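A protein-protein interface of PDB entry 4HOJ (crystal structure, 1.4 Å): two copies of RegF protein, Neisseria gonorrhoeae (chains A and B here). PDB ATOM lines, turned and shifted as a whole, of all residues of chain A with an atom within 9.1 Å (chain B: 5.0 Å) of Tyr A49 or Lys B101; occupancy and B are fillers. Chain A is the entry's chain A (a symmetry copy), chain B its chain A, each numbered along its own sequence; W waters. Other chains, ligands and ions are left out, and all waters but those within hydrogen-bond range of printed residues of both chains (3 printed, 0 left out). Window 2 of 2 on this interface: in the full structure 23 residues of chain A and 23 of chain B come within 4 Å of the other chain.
Pro A48 touches Arg B98 (CG to CZ, 3.6 Å).
Tyr A49 touches Arg B98.
Lys B101 touches Tyr A49 (CD to OH, 3.4 Å).
Arg B98 touches His A63.
Tyr B97 touches Ile A67 (CB to CD1, 3.4 Å).
Water W2 lies within hydrogen-bond range of the side-chain hydroxyl (OH) of Tyr B97 (2.6 Å), the side-chain amino group (NZ) of Lys B101 (2.7 Å) and the side-chain carboxylate (OE1) of Glu A64 (3.5 Å).
Water W1 lies within hydrogen-bond range of the side-chain carboxylate of Glu A64 (2.7 Å) and the side-chain hydroxyl of Tyr B97 (3.3 Å).
Water W3 bridges NE2 of His A63 and NH1 of Arg B98.
OE1 of Glu A64 is in hydrogen-bond range of OH of Tyr B97.
The side-chain hydroxyl (OH) of Tyr A49 sits close to the side-chain carboxylate (OE2) of Glu B102, 2.2 Å away.
No position is printed for both chains.
Hydrophobic or aromatic side chains of chain A that line the printed part of chain B: Pro A48, Tyr A49, His A63 and Ile A67.
Printed residues of chain B that touch a printed residue of chain A: Tyr B97, Arg B98, Lys B101 and Glu B102.
Hydrophobic or aromatic side chains of chain B that line the printed part of chain A: Tyr B97.
Among the printed residues, no Asp or Glu carboxylate lies within 4 Å of a Lys or Arg side-chain nitrogen of the other chain.
NE of Arg B98 is in salt-bridge range of OE2 of Glu B102 (2.8 Å).
The backbone carbonyl oxygen (O) of Lys B101 lies close to the side-chain amide oxygen (OD1) of Asn B105 (3.1 Å).
OD1 of Asn A47 sits at hydrogen-bond distance from N of Tyr A49 (2.9 Å).
The side-chain amide oxygen (OD1) of Asn A47 sits close to a ring nitrogen (ND1) of His A63 (3.4 Å).
Lys B101 touches just one residue of chain A: Tyr A49 (3.4 Å).
Of the printed residues of chain A, Glu B102 touches Tyr A49.
Of the printed residues of chain B, His A63 touches Arg B98.
Printed residues of chain B within 4 Å of Glu A64: Tyr B97.
Of the printed residues of chain A, Arg B98 touches Pro A48 (3.6 Å), Tyr A49 (3.8 Å) and His A63 (3.9 Å).
The nearest printed residue of chain A that does not touch Arg B98 is Ile A67 (6.2 Å).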
ATOM      1  N   LYS A  39      13.476 -26.442  39.103  1.00  0.00           N
ATOM      2  CA  LYS A  39      13.690 -26.362  37.659  1.00  0.00           C
ATOM      3  C   LYS A  39      12.609 -27.091  36.874  1.00  0.00           C
ATOM      4  O   LYS A  39      12.126 -28.148  37.292  1.00  0.00           O
ATOM      5  CB  LYS A  39      15.014 -27.001  37.292  1.00  0.00           C
ATOM      6  CG  LYS A  39      16.169 -26.331  37.913  1.00  0.00           C
ATOM      7  CD  LYS A  39      17.366 -27.340  37.756  1.00  0.00           C
ATOM      8  CE  LYS A  39      18.611 -26.781  38.347  1.00  0.00           C
ATOM      9  NZ  LYS A  39      19.624 -27.917  38.294  1.00  0.00           N
ATOM     10  N   LEU A  43      14.229 -27.820  31.119  1.00  0.00           N
ATOM     11  CA  LEU A  43      15.593 -27.330  31.258  1.00  0.00           C
ATOM     12  C   LEU A  43      16.628 -28.418  30.928  1.00  0.00           C
ATOM     13  O   LEU A  43      17.607 -28.140  30.211  1.00  0.00           O
ATOM     14  CB  LEU A  43      15.861 -26.720  32.637  1.00  0.00           C
ATOM     15  CG  LEU A  43      17.168 -25.937  32.700  1.00  0.00           C
ATOM     16  CD1 LEU A  43      17.198 -24.639  31.818  1.00  0.00           C
ATOM     17  CD2 LEU A  43      17.539 -25.539  34.132  1.00  0.00           C
ATOM     18  N   ALA A  44      16.437 -29.628  31.423  1.00  0.00           N
ATOM     19  CA  ALA A  44      17.400 -30.684  31.126  1.00  0.00           C
ATOM     20  C   ALA A  44      17.312 -31.188  29.679  1.00  0.00           C
ATOM     21  O   ALA A  44      18.272 -31.763  29.182  1.00  0.00           O
ATOM     22  CB  ALA A  44      17.247 -31.815  32.113  1.00  0.00           C
ATOM     23  N   VAL A  45      16.191 -30.986  28.998  1.00  0.00           N
ATOM     24  CA  VAL A  45      16.102 -31.361  27.591  1.00  0.00           C
ATOM     25  C   VAL A  45      16.910 -30.350  26.768  1.00  0.00           C
ATOM     26  O   VAL A  45      17.608 -30.722  25.811  1.00  0.00           O
ATOM     27  CB  VAL A  45      14.637 -31.360  27.149  1.00  0.00           C
ATOM     28  CG1 VAL A  45      14.527 -31.682  25.648  1.00  0.00           C
ATOM     29  CG2 VAL A  45      13.850 -32.416  27.940  1.00  0.00           C
ATOM     30  N   MET A  46      16.841 -29.074  27.132  1.00  0.00           N
ATOM     31  CA  MET A  46      17.578 -28.016  26.426  1.00  0.00           C
ATOM     32  C   MET A  46      19.067 -28.057  26.745  1.00  0.00           C
ATOM     33  O   MET A  46      19.909 -27.681  25.923  1.00  0.00           O
ATOM     34  CB  MET A  46      17.021 -26.623  26.812  1.00  0.00           C
ATOM     35  CG  MET A  46      15.647 -26.317  26.207  1.00  0.00           C
ATOM     36  SD  MET A  46      15.039 -24.689  26.581  1.00  0.00           S
ATOM     37  CE  MET A  46      14.835 -24.821  28.352  1.00  0.00           C
ATOM     38  N   ASN A  47      19.418 -28.433  27.956  1.00  0.00           N
ATOM     39  CA  ASN A  47      20.775 -28.316  28.432  1.00  0.00           C
ATOM     40  C   ASN A  47      21.064 -29.588  29.223  1.00  0.00           C
ATOM     41  O   ASN A  47      20.529 -29.774  30.304  1.00  0.00           O
ATOM     42  CB  ASN A  47      20.912 -27.079  29.349  1.00  0.00           C
ATOM     43  CG  ASN A  47      22.324 -26.932  29.916  1.00  0.00           C
ATOM     44  OD1 ASN A  47      23.210 -27.785  29.654  1.00  0.00           O
ATOM     45  ND2 ASN A  47      22.558 -25.906  30.697  1.00  0.00           N
ATOM     46  N   PRO A  48      21.956 -30.463  28.739  1.00  0.00           N
ATOM     47  CA  PRO A  48      22.176 -31.702  29.509  1.00  0.00           C
ATOM     48  C   PRO A  48      22.801 -31.476  30.874  1.00  0.00           C
ATOM     49  O   PRO A  48      22.682 -32.344  31.753  1.00  0.00           O
ATOM     50  CB  PRO A  48      23.138 -32.513  28.617  1.00  0.00           C
ATOM     51  CG  PRO A  48      23.844 -31.511  27.865  1.00  0.00           C
ATOM     52  CD  PRO A  48      22.822 -30.406  27.545  1.00  0.00           C
ATOM     53  N   TYR A  49      23.362 -30.288  31.103  1.00  0.00           N
ATOM     54  CA  TYR A  49      23.849 -29.960  32.439  1.00  0.00           C
ATOM     55  C   TYR A  49      22.786 -29.395  33.375  1.00  0.00           C
ATOM     56  O   TYR A  49      23.080 -29.174  34.545  1.00  0.00           O
ATOM     57  CB  TYR A  49      25.030 -28.989  32.357  1.00  0.00           C
ATOM     58  CG  TYR A  49      26.088 -29.489  31.412  1.00  0.00           C
ATOM     59  CD1 TYR A  49      26.664 -30.735  31.577  1.00  0.00           C
ATOM     60  CD2 TYR A  49      26.459 -28.758  30.301  1.00  0.00           C
ATOM     61  CE1 TYR A  49      27.621 -31.194  30.673  1.00  0.00           C
ATOM     62  CE2 TYR A  49      27.414 -29.217  29.402  1.00  0.00           C
ATOM     63  CZ  TYR A  49      27.967 -30.416  29.606  1.00  0.00           C
ATOM     64  OH  TYR A  49      28.930 -30.858  28.665  1.00  0.00           O
ATOM     65  N   ASN A  50      21.581 -29.189  32.830  1.00  0.00           N
ATOM     66  CA  ASN A  50      20.436 -28.776  33.674  1.00  0.00           C
ATOM     67  C   ASN A  50      20.675 -27.482  34.457  1.00  0.00           C
ATOM     68  O   ASN A  50      20.427 -27.401  35.664  1.00  0.00           O
ATOM     69  CB  ASN A  50      20.076 -29.896  34.622  1.00  0.00           C
ATOM     70  CG  ASN A  50      18.679 -29.767  35.182  1.00  0.00           C
ATOM     71  OD1 ASN A  50      17.808 -29.127  34.597  1.00  0.00           O
ATOM     72  ND2 ASN A  50      18.441 -30.468  36.276  1.00  0.00           N
ATOM     73  N   GLN A  51      21.223 -26.485  33.767  1.00  0.00           N
ATOM     74  CA  GLN A  51      21.584 -25.190  34.311  1.00  0.00           C
ATOM     75  C   GLN A  51      21.024 -24.075  33.429  1.00  0.00           C
ATOM     76  O   GLN A  51      20.720 -24.235  32.245  1.00  0.00           O
ATOM     77  CB  GLN A  51      23.098 -25.019  34.347  1.00  0.00           C
ATOM     78  CG  GLN A  51      23.758 -25.962  35.325  1.00  0.00           C
ATOM     79  CD  GLN A  51      25.252 -25.777  35.343  1.00  0.00           C
ATOM     80  OE1 GLN A  51      25.864 -25.465  34.313  1.00  0.00           O
ATOM     81  NE2 GLN A  51      25.865 -25.925  36.521  1.00  0.00           N
ATOM     82  N   VAL A  52      20.926 -22.900  34.073  1.00  0.00           N
ATOM     83  CA  VAL A  52      20.767 -21.646  33.337  1.00  0.00           C
ATOM     84  C   VAL A  52      22.122 -20.941  33.250  1.00  0.00           C
ATOM     85  O   VAL A  52      22.992 -21.168  34.093  1.00  0.00           O
ATOM     86  CB  VAL A  52      19.730 -20.703  34.037  1.00  0.00           C
ATOM     87  CG1 VAL A  52      18.371 -21.321  33.880  1.00  0.00           C
ATOM     88  CG2 VAL A  52      20.107 -20.467  35.504  1.00  0.00           C
ATOM     89  N   PRO A  53      22.333 -20.105  32.231  1.00  0.00           N
ATOM     90  CA  PRO A  53      21.354 -19.712  31.220  1.00  0.00           C
ATOM     91  C   PRO A  53      21.273 -20.654  30.039  1.00  0.00           C
ATOM     92  O   PRO A  53      22.207 -21.456  29.723  1.00  0.00           O
ATOM     93  CB  PRO A  53      21.908 -18.379  30.710  1.00  0.00           C
ATOM     94  CG  PRO A  53      23.450 -18.512  30.909  1.00  0.00           C
ATOM     95  CD  PRO A  53      23.523 -19.237  32.261  1.00  0.00           C
ATOM     96  N   VAL A  54      20.142 -20.599  29.328  1.00  0.00           N
ATOM     97  CA  VAL A  54      19.934 -21.238  28.026  1.00  0.00           C
ATOM     98  C   VAL A  54      19.369 -20.170  27.096  1.00  0.00           C
ATOM     99  O   VAL A  54      18.542 -19.325  27.537  1.00  0.00           O
ATOM    100  CB  VAL A  54      18.942 -22.382  28.142  1.00  0.00           C
ATOM    101  CG1 VAL A  54      18.521 -22.940  26.781  1.00  0.00           C
ATOM    102  CG2 VAL A  54      19.568 -23.501  29.003  1.00  0.00           C
ATOM    103  N   LEU A  62      21.173 -22.979  22.730  1.00  0.00           N
ATOM    104  CA  LEU A  62      22.538 -22.871  23.256  1.00  0.00           C
ATOM    105  C   LEU A  62      22.530 -22.829  24.760  1.00  0.00           C
ATOM    106  O   LEU A  62      21.663 -22.185  25.373  1.00  0.00           O
ATOM    107  CB  LEU A  62      23.205 -21.598  22.765  1.00  0.00           C
ATOM    108  CG  LEU A  62      23.420 -21.498  21.264  1.00  0.00           C
ATOM    109  CD1 LEU A  62      24.019 -20.109  20.978  1.00  0.00           C
ATOM    110  CD2 LEU A  62      24.408 -22.579  20.769  1.00  0.00           C
ATOM    111  N   HIS A  63      23.528 -23.428  25.405  1.00  0.00           N
ATOM    112  CA  HIS A  63      23.841 -23.148  26.800  1.00  0.00           C
ATOM    113  C   HIS A  63      25.318 -22.741  26.824  1.00  0.00           C
ATOM    114  O   HIS A  63      25.971 -22.668  25.773  1.00  0.00           O
ATOM    115  CB  HIS A  63      23.530 -24.374  27.676  1.00  0.00           C
ATOM    116  CG  HIS A  63      24.142 -25.665  27.191  1.00  0.00           C
ATOM    117  ND1 HIS A  63      25.378 -26.135  27.603  1.00  0.00           N
ATOM    118  CD2 HIS A  63      23.660 -26.593  26.331  1.00  0.00           C
ATOM    119  CE1 HIS A  63      25.635 -27.282  26.983  1.00  0.00           C
ATOM    120  NE2 HIS A  63      24.611 -27.584  26.202  1.00  0.00           N
ATOM    121  N   GLU A  64      25.794 -22.487  28.038  1.00  0.00           N
ATOM    122  CA  GLU A  64      27.111 -21.948  28.358  1.00  0.00           C
ATOM    123  C   GLU A  64      27.152 -20.472  28.032  1.00  0.00           C
ATOM    124  O   GLU A  64      27.186 -20.023  26.870  1.00  0.00           O
ATOM    125  CB  GLU A  64      28.206 -22.701  27.594  1.00  0.00           C
ATOM    126  CG  GLU A  64      29.614 -22.360  28.066  1.00  0.00           C
ATOM    127  CD  GLU A  64      29.922 -22.754  29.491  1.00  0.00           C
ATOM    128  OE1 GLU A  64      29.142 -23.479  30.113  1.00  0.00           O
ATOM    129  OE2 GLU A  64      31.052 -22.390  29.917  1.00  0.00           O
ATOM    130  N   ILE A  67      29.321 -18.805  25.380  1.00  0.00           N
ATOM    131  CA  ILE A  67      29.009 -19.276  24.009  1.00  0.00           C
ATOM    132  C   ILE A  67      27.713 -18.579  23.540  1.00  0.00           C
ATOM    133  O   ILE A  67      27.612 -18.105  22.399  1.00  0.00           O
ATOM    134  CB  ILE A  67      28.849 -20.811  24.016  1.00  0.00           C
ATOM    135  CG1 ILE A  67      30.221 -21.416  24.258  1.00  0.00           C
ATOM    136  CG2 ILE A  67      28.287 -21.293  22.703  1.00  0.00           C
ATOM    137  CD1 ILE A  67      30.212 -22.888  24.229  1.00  0.00           C
ATOM    138  N   GLN A 108      31.385 -20.778  40.881  1.00  0.00           N
ATOM    139  CA  GLN A 108      30.450 -21.908  40.954  1.00  0.00           C
ATOM    140  C   GLN A 108      30.379 -22.559  42.320  1.00  0.00           C
ATOM    141  O   GLN A 108      29.313 -23.055  42.721  1.00  0.00           O
ATOM    142  CB  GLN A 108      30.796 -22.965  39.880  1.00  0.00           C
ATOM    143  CG  GLN A 108      30.548 -22.408  38.449  1.00  0.00           C
ATOM    144  CD  GLN A 108      30.911 -23.392  37.346  1.00  0.00           C
ATOM    145  OE1 GLN A 108      30.336 -24.484  37.273  1.00  0.00           O
ATOM    146  NE2 GLN A 108      31.909 -23.053  36.544  1.00  0.00           N
ATOM    147  N   TYR B  97      32.776 -27.113  22.960  1.00  0.00           N
ATOM    148  CA  TYR B  97      32.779 -27.021  24.406  1.00  0.00           C
ATOM    149  C   TYR B  97      32.385 -28.374  24.994  1.00  0.00           C
ATOM    150  O   TYR B  97      33.036 -28.857  25.947  1.00  0.00           O
ATOM    151  CB  TYR B  97      31.773 -25.903  24.840  1.00  0.00           C
ATOM    152  CG  TYR B  97      31.634 -25.860  26.359  1.00  0.00           C
ATOM    153  CD1 TYR B  97      32.548 -25.172  27.155  1.00  0.00           C
ATOM    154  CD2 TYR B  97      30.611 -26.494  26.984  1.00  0.00           C
ATOM    155  CE1 TYR B  97      32.459 -25.168  28.562  1.00  0.00           C
ATOM    156  CE2 TYR B  97      30.488 -26.474  28.394  1.00  0.00           C
ATOM    157  CZ  TYR B  97      31.442 -25.850  29.170  1.00  0.00           C
ATOM    158  OH  TYR B  97      31.386 -25.860  30.536  1.00  0.00           O
ATOM    159  N   ARG B  98      31.320 -28.998  24.484  1.00  0.00           N
ATOM    160  CA  ARG B  98      30.943 -30.288  25.035  1.00  0.00           C
ATOM    161  C   ARG B  98      32.006 -31.357  24.795  1.00  0.00           C
ATOM    162  O   ARG B  98      32.187 -32.215  25.665  1.00  0.00           O
ATOM    163  CB  ARG B  98      29.601 -30.720  24.484  1.00  0.00           C
ATOM    164  CG  ARG B  98      28.489 -29.795  25.069  1.00  0.00           C
ATOM    165  CD  ARG B  98      27.094 -30.340  24.963  1.00  0.00           C
ATOM    166  NE  ARG B  98      27.011 -31.675  25.520  1.00  0.00           N
ATOM    167  CZ  ARG B  98      26.067 -32.540  25.194  1.00  0.00           C
ATOM    168  NH1 ARG B  98      25.069 -32.145  24.383  1.00  0.00           N
ATOM    169  NH2 ARG B  98      26.104 -33.764  25.718  1.00  0.00           N
ATOM    170  N   MET B  99      32.694 -31.358  23.652  1.00  0.00           N
ATOM    171  CA  MET B  99      33.805 -32.311  23.477  1.00  0.00           C
ATOM    172  C   MET B  99      34.902 -32.067  24.488  1.00  0.00           C
ATOM    173  O   MET B  99      35.482 -33.011  25.026  1.00  0.00           O
ATOM    174  CB  MET B  99      34.375 -32.249  22.073  1.00  0.00           C
ATOM    175  CG  MET B  99      33.391 -32.684  20.995  1.00  0.00           C
ATOM    176  SD  MET B  99      34.238 -33.104  19.474  1.00  0.00           S
ATOM    177  CE  MET B  99      34.798 -31.476  18.974  1.00  0.00           C
ATOM    178  N   GLU B 100      35.212 -30.817  24.831  1.00  0.00           N
ATOM    179  CA  GLU B 100      36.248 -30.545  25.802  1.00  0.00           C
ATOM    180  C   GLU B 100      35.864 -31.067  27.125  1.00  0.00           C
ATOM    181  O   GLU B 100      36.689 -31.625  27.867  1.00  0.00           O
ATOM    182  CB  GLU B 100      36.647 -29.044  25.935  1.00  0.00           C
ATOM    183  CG  GLU B 100      37.617 -28.394  24.909  1.00  0.00           C
ATOM    184  CD  GLU B 100      38.803 -29.253  24.277  1.00  0.00           C
ATOM    185  OE1 GLU B 100      40.029 -28.976  24.408  1.00  0.00           O
ATOM    186  OE2 GLU B 100      38.422 -30.136  23.622  1.00  0.00           O
ATOM    187  N   LYS B 101      34.588 -30.900  27.498  1.00  0.00           N
ATOM    188  CA  LYS B 101      34.147 -31.256  28.849  1.00  0.00           C
ATOM    189  C   LYS B 101      33.821 -32.754  29.027  1.00  0.00           C
ATOM    190  O   LYS B 101      33.877 -33.257  30.138  1.00  0.00           O
ATOM    191  CB  LYS B 101      32.894 -30.424  29.184  1.00  0.00           C
ATOM    192  CG  LYS B 101      32.219 -30.752  30.502  1.00  0.00           C
ATOM    193  CD  LYS B 101      31.249 -29.647  30.901  1.00  0.00           C
ATOM    194  CE  LYS B 101      30.516 -30.039  32.159  1.00  0.00           C
ATOM    195  NZ  LYS B 101      29.681 -28.955  32.739  1.00  0.00           N
ATOM    196  N   GLU B 102      33.479 -33.425  27.924  1.00  0.00           N
ATOM    197  CA  GLU B 102      32.949 -34.806  28.004  1.00  0.00           C
ATOM    198  C   GLU B 102      33.824 -35.842  27.318  1.00  0.00           C
ATOM    199  O   GLU B 102      33.616 -37.056  27.530  1.00  0.00           O
ATOM    200  CB  GLU B 102      31.547 -34.857  27.382  1.00  0.00           C
ATOM    201  CG  GLU B 102      30.577 -33.899  28.037  1.00  0.00           C
ATOM    202  CD  GLU B 102      29.282 -33.754  27.275  1.00  0.00           C
ATOM    203  OE1 GLU B 102      28.997 -34.580  26.394  1.00  0.00           O
ATOM    204  OE2 GLU B 102      28.568 -32.762  27.545  1.00  0.00           O
ATOM    205  N   LEU B 103      34.759 -35.427  26.482  1.00  0.00           N
ATOM    206  CA  LEU B 103      35.688 -36.372  25.808  1.00  0.00           C
ATOM    207  C   LEU B 103      37.124 -36.057  26.146  1.00  0.00           C
ATOM    208  O   LEU B 103      37.878 -36.933  26.578  1.00  0.00           O
ATOM    209  CB  LEU B 103      35.500 -36.330  24.296  1.00  0.00           C
ATOM    210  CG  LEU B 103      34.198 -36.901  23.743  1.00  0.00           C
ATOM    211  CD1 LEU B 103      34.157 -36.627  22.244  1.00  0.00           C
ATOM    212  CD2 LEU B 103      34.080 -38.425  24.018  1.00  0.00           C
ATOM    213  N   ASN B 105      38.457 -34.238  28.462  1.00  0.00           N
ATOM    214  CA  ASN B 105      38.829 -34.376  29.887  1.00  0.00           C
ATOM    215  C   ASN B 105      39.366 -35.789  30.131  1.00  0.00           C
ATOM    216  O   ASN B 105      40.366 -35.983  30.812  1.00  0.00           O
ATOM    217  CB  ASN B 105      37.619 -34.082  30.759  1.00  0.00           C
ATOM    218  CG  ASN B 105      36.442 -34.988  30.451  1.00  0.00           C
ATOM    219  OD1 ASN B 105      36.126 -35.281  29.291  1.00  0.00           O
ATOM    220  ND2 ASN B 105      35.759 -35.469  31.538  1.00  0.00           N
HETATM  221  O   HOH W   1      32.731 -23.144  31.832  1.00  0.00           O
HETATM  222  O   HOH W   2      29.060 -26.684  31.469  1.00  0.00           O
HETATM  223  O   HOH W   3      24.156 -29.290  24.044  1.00  0.00           O
